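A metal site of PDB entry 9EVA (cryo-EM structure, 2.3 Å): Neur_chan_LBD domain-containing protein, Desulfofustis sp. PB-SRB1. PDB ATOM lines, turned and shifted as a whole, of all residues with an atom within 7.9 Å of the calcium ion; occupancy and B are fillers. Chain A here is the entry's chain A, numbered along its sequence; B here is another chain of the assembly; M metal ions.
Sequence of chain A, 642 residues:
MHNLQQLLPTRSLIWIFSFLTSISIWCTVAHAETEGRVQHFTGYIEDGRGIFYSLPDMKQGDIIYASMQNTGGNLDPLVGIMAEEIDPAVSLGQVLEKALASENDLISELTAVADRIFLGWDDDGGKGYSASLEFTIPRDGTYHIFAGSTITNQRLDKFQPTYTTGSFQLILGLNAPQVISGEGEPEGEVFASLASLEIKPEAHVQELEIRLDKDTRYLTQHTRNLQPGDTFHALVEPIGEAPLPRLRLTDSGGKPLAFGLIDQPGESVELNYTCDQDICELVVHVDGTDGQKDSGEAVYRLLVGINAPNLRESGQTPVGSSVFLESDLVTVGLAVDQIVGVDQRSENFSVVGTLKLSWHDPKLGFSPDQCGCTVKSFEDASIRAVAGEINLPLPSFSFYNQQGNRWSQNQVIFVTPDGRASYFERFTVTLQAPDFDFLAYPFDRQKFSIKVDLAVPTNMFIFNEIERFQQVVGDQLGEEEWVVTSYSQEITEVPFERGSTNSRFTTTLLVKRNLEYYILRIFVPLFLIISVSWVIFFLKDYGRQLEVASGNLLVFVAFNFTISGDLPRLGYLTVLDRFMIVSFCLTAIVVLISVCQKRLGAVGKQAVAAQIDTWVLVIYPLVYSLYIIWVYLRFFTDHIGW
The backbone carbonyl oxygen of Glu 347 is in hydrogen-bond range of the backbone NH of Ala 433 (2.9 Å).
Of the 16 residues printed, 4 come within 4 Å of the calcium ion.
The calcium ion is bound by O of Pro 434 (2.5 Å). O of Leu 477 of chain B binds the calcium ion, 2.5 Å away. O of Phe 436 binds the calcium ion (2.5 Å). The side-chain carboxylate (OE1) of Glu 347 is bound to the calcium ion (2.7 Å). Slightly farther from the calcium ion lies the side-chain carboxylate (OE2) of Glu 347 (3.1 Å).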
ATOM      1  N   GLN A 344      15.775  25.156 -14.363  1.00  0.00           N
ATOM      2  CA  GLN A 344      15.868  24.333 -15.569  1.00  0.00           C
ATOM      3  C   GLN A 344      15.625  22.856 -15.312  1.00  0.00           C
ATOM      4  O   GLN A 344      15.410  22.109 -16.267  1.00  0.00           O
ATOM      5  CB  GLN A 344      17.227  24.533 -16.226  1.00  0.00           C
ATOM      6  CG  GLN A 344      17.491  25.956 -16.679  1.00  0.00           C
ATOM      7  CD  GLN A 344      18.862  26.138 -17.299  1.00  0.00           C
ATOM      8  OE1 GLN A 344      19.170  27.193 -17.838  1.00  0.00           O
ATOM      9  NE2 GLN A 344      19.686  25.109 -17.221  1.00  0.00           N
ATOM     10  N   GLU A 347      11.570  23.018 -14.381  1.00  0.00           N
ATOM     11  CA  GLU A 347      10.877  23.702 -15.462  1.00  0.00           C
ATOM     12  C   GLU A 347       9.815  24.670 -14.935  1.00  0.00           C
ATOM     13  O   GLU A 347       8.610  24.507 -15.153  1.00  0.00           O
ATOM     14  CB  GLU A 347      10.283  22.692 -16.453  1.00  0.00           C
ATOM     15  CG  GLU A 347      11.307  21.749 -17.054  1.00  0.00           C
ATOM     16  CD  GLU A 347      10.778  20.961 -18.229  1.00  0.00           C
ATOM     17  OE1 GLU A 347       9.719  21.347 -18.770  1.00  0.00           O
ATOM     18  OE2 GLU A 347      11.420  19.962 -18.618  1.00  0.00           O
ATOM     19  N   ALA A 433       6.257  25.718 -16.241  1.00  0.00           N
ATOM     20  CA  ALA A 433       6.458  25.834 -17.683  1.00  0.00           C
ATOM     21  C   ALA A 433       6.961  24.528 -18.274  1.00  0.00           C
ATOM     22  O   ALA A 433       8.136  24.421 -18.634  1.00  0.00           O
ATOM     23  CB  ALA A 433       7.440  26.961 -17.997  1.00  0.00           C
ATOM     24  N   PRO A 434       6.102  23.508 -18.398  1.00  0.00           N
ATOM     25  CA  PRO A 434       6.565  22.226 -18.964  1.00  0.00           C
ATOM     26  C   PRO A 434       6.916  22.292 -20.446  1.00  0.00           C
ATOM     27  O   PRO A 434       7.454  21.323 -20.983  1.00  0.00           O
ATOM     28  CB  PRO A 434       5.381  21.294 -18.710  1.00  0.00           C
ATOM     29  CG  PRO A 434       4.198  22.195 -18.610  1.00  0.00           C
ATOM     30  CD  PRO A 434       4.699  23.444 -17.964  1.00  0.00           C
ATOM     31  N   ASP A 435       6.619  23.404 -21.129  1.00  0.00           N
ATOM     32  CA  ASP A 435       6.923  23.523 -22.545  1.00  0.00           C
ATOM     33  C   ASP A 435       8.403  23.763 -22.837  1.00  0.00           C
ATOM     34  O   ASP A 435       8.783  23.788 -24.004  1.00  0.00           O
ATOM     35  CB  ASP A 435       6.088  24.642 -23.173  1.00  0.00           C
ATOM     36  CG  ASP A 435       4.605  24.306 -23.205  1.00  0.00           C
ATOM     37  OD1 ASP A 435       4.224  23.215 -22.733  1.00  0.00           O
ATOM     38  OD2 ASP A 435       3.822  25.139 -23.701  1.00  0.00           O
ATOM     39  N   PHE A 436       9.231  23.966 -21.805  1.00  0.00           N
ATOM     40  CA  PHE A 436      10.655  24.192 -22.012  1.00  0.00           C
ATOM     41  C   PHE A 436      11.308  23.037 -22.758  1.00  0.00           C
ATOM     42  O   PHE A 436      10.956  21.865 -22.548  1.00  0.00           O
ATOM     43  CB  PHE A 436      11.363  24.395 -20.670  1.00  0.00           C
ATOM     44  CG  PHE A 436      11.136  25.741 -20.044  1.00  0.00           C
ATOM     45  CD1 PHE A 436      10.648  26.795 -20.791  1.00  0.00           C
ATOM     46  CD2 PHE A 436      11.424  25.948 -18.711  1.00  0.00           C
ATOM     47  CE1 PHE A 436      10.436  28.031 -20.214  1.00  0.00           C
ATOM     48  CE2 PHE A 436      11.226  27.185 -18.130  1.00  0.00           C
ATOM     49  CZ  PHE A 436      10.732  28.226 -18.882  1.00  0.00           C
ATOM     50  N   ASP A 437      12.252  23.368 -23.634  1.00  0.00           N
ATOM     51  CA  ASP A 437      13.014  22.369 -24.382  1.00  0.00           C
ATOM     52  C   ASP A 437      14.468  22.849 -24.475  1.00  0.00           C
ATOM     53  O   ASP A 437      14.749  23.826 -25.174  1.00  0.00           O
ATOM     54  CB  ASP A 437      12.426  22.147 -25.771  1.00  0.00           C
ATOM     55  CG  ASP A 437      13.118  21.038 -26.532  1.00  0.00           C
ATOM     56  OD1 ASP A 437      13.929  20.302 -25.933  1.00  0.00           O
ATOM     57  OD2 ASP A 437      12.856  20.892 -27.746  1.00  0.00           O
ATOM     58  N   PHE A 438      15.375  22.155 -23.788  1.00  0.00           N
ATOM     59  CA  PHE A 438      16.771  22.551 -23.707  1.00  0.00           C
ATOM     60  C   PHE A 438      17.682  21.685 -24.578  1.00  0.00           C
ATOM     61  O   PHE A 438      18.877  21.572 -24.268  1.00  0.00           O
ATOM     62  CB  PHE A 438      17.253  22.523 -22.257  1.00  0.00           C
ATOM     63  CG  PHE A 438      16.468  23.409 -21.343  1.00  0.00           C
ATOM     64  CD1 PHE A 438      16.577  24.781 -21.435  1.00  0.00           C
ATOM     65  CD2 PHE A 438      15.625  22.864 -20.391  1.00  0.00           C
ATOM     66  CE1 PHE A 438      15.856  25.600 -20.592  1.00  0.00           C
ATOM     67  CE2 PHE A 438      14.905  23.684 -19.548  1.00  0.00           C
ATOM     68  CZ  PHE A 438      15.022  25.053 -19.644  1.00  0.00           C
ATOM     69  N   GLN A 446      13.327  30.050 -25.908  1.00  0.00           N
ATOM     70  CA  GLN A 446      12.235  29.649 -25.042  1.00  0.00           C
ATOM     71  C   GLN A 446      11.124  30.690 -25.062  1.00  0.00           C
ATOM     72  O   GLN A 446      11.302  31.817 -25.532  1.00  0.00           O
ATOM     73  CB  GLN A 446      12.722  29.433 -23.594  1.00  0.00           C
ATOM     74  CG  GLN A 446      13.920  28.515 -23.454  1.00  0.00           C
ATOM     75  CD  GLN A 446      13.633  27.088 -23.896  1.00  0.00           C
ATOM     76  OE1 GLN A 446      12.504  26.622 -23.844  1.00  0.00           O
ATOM     77  NE2 GLN A 446      14.667  26.386 -24.343  1.00  0.00           N
ATOM     78  N   TYR A 572      19.740  14.219 -19.774  1.00  0.00           N
ATOM     79  CA  TYR A 572      19.749  13.928 -21.202  1.00  0.00           C
ATOM     80  C   TYR A 572      20.769  14.833 -21.874  1.00  0.00           C
ATOM     81  O   TYR A 572      21.159  15.863 -21.322  1.00  0.00           O
ATOM     82  CB  TYR A 572      18.353  14.083 -21.827  1.00  0.00           C
ATOM     83  CG  TYR A 572      17.655  15.381 -21.488  1.00  0.00           C
ATOM     84  CD1 TYR A 572      17.845  16.519 -22.260  1.00  0.00           C
ATOM     85  CD2 TYR A 572      16.807  15.466 -20.393  1.00  0.00           C
ATOM     86  CE1 TYR A 572      17.211  17.698 -21.958  1.00  0.00           C
ATOM     87  CE2 TYR A 572      16.164  16.639 -20.083  1.00  0.00           C
ATOM     88  CZ  TYR A 572      16.366  17.759 -20.868  1.00  0.00           C
ATOM     89  OH  TYR A 572      15.737  18.942 -20.557  1.00  0.00           O
ATOM     90  N   GLN B 338       2.772  16.029 -15.023  1.00  0.00           N
ATOM     91  CA  GLN B 338       4.218  16.209 -15.030  1.00  0.00           C
ATOM     92  C   GLN B 338       4.832  15.633 -13.765  1.00  0.00           C
ATOM     93  O   GLN B 338       4.282  15.817 -12.670  1.00  0.00           O
ATOM     94  CB  GLN B 338       4.573  17.704 -15.150  1.00  0.00           C
ATOM     95  CG  GLN B 338       6.062  17.993 -15.151  1.00  0.00           C
ATOM     96  CD  GLN B 338       6.366  19.485 -15.085  1.00  0.00           C
ATOM     97  OE1 GLN B 338       5.463  20.300 -14.937  1.00  0.00           O
ATOM     98  NE2 GLN B 338       7.635  19.826 -15.202  1.00  0.00           N
ATOM     99  N   GLN B 476       4.631  15.978 -23.019  1.00  0.00           N
ATOM    100  CA  GLN B 476       5.183  17.317 -22.861  1.00  0.00           C
ATOM    101  C   GLN B 476       6.313  17.511 -23.872  1.00  0.00           C
ATOM    102  O   GLN B 476       7.002  16.554 -24.232  1.00  0.00           O
ATOM    103  CB  GLN B 476       5.709  17.546 -21.440  1.00  0.00           C
ATOM    104  CG  GLN B 476       4.665  17.439 -20.342  1.00  0.00           C
ATOM    105  CD  GLN B 476       3.650  18.574 -20.379  1.00  0.00           C
ATOM    106  OE1 GLN B 476       3.853  19.582 -21.071  1.00  0.00           O
ATOM    107  NE2 GLN B 476       2.571  18.427 -19.633  1.00  0.00           N
ATOM    108  N   LEU B 477       6.488  18.750 -24.312  1.00  0.00           N
ATOM    109  CA  LEU B 477       7.553  19.062 -25.260  1.00  0.00           C
ATOM    110  C   LEU B 477       8.917  18.911 -24.607  1.00  0.00           C
ATOM    111  O   LEU B 477       9.096  19.215 -23.421  1.00  0.00           O
ATOM    112  CB  LEU B 477       7.397  20.490 -25.795  1.00  0.00           C
ATOM    113  CG  LEU B 477       6.174  20.786 -26.670  1.00  0.00           C
ATOM    114  CD1 LEU B 477       6.068  22.276 -26.955  1.00  0.00           C
ATOM    115  CD2 LEU B 477       6.233  19.993 -27.966  1.00  0.00           C
ATOM    116  N   GLY B 478       9.885  18.441 -25.386  1.00  0.00           N
ATOM    117  CA  GLY B 478      11.228  18.223 -24.889  1.00  0.00           C
ATOM    118  C   GLY B 478      11.406  16.862 -24.247  1.00  0.00           C
ATOM    119  O   GLY B 478      10.483  16.073 -24.099  1.00  0.00           O
ATOM    120  N   GLU B 479      12.653  16.594 -23.857  1.00  0.00           N
ATOM    121  CA  GLU B 479      12.989  15.329 -23.220  1.00  0.00           C
ATOM    122  C   GLU B 479      12.742  15.406 -21.719  1.00  0.00           C
ATOM    123  O   GLU B 479      12.695  16.480 -21.110  1.00  0.00           O
ATOM    124  CB  GLU B 479      14.456  14.969 -23.487  1.00  0.00           C
ATOM    125  CG  GLU B 479      14.848  14.977 -24.944  1.00  0.00           C
ATOM    126  CD  GLU B 479      14.165  13.887 -25.757  1.00  0.00           C
ATOM    127  OE1 GLU B 479      13.770  12.864 -25.157  1.00  0.00           O
ATOM    128  OE2 GLU B 479      14.027  14.055 -26.981  1.00  0.00           O
ATOM    129  N   GLU B 480      12.578  14.226 -21.115  1.00  0.00           N
ATOM    130  CA  GLU B 480      12.408  14.098 -19.673  1.00  0.00           C
ATOM    131  C   GLU B 480      13.470  13.150 -19.118  1.00  0.00           C
ATOM    132  O   GLU B 480      13.979  12.275 -19.822  1.00  0.00           O
ATOM    133  CB  GLU B 480      11.007  13.566 -19.311  1.00  0.00           C
ATOM    134  CG  GLU B 480       9.892  14.596 -19.432  1.00  0.00           C
ATOM    135  CD  GLU B 480       9.451  14.827 -20.863  1.00  0.00           C
ATOM    136  OE1 GLU B 480       9.758  13.982 -21.732  1.00  0.00           O
ATOM    137  OE2 GLU B 480       8.790  15.851 -21.127  1.00  0.00           O
HETATM  138 CA    CA M   1       9.650  20.198 -21.186  1.00  0.00          CA
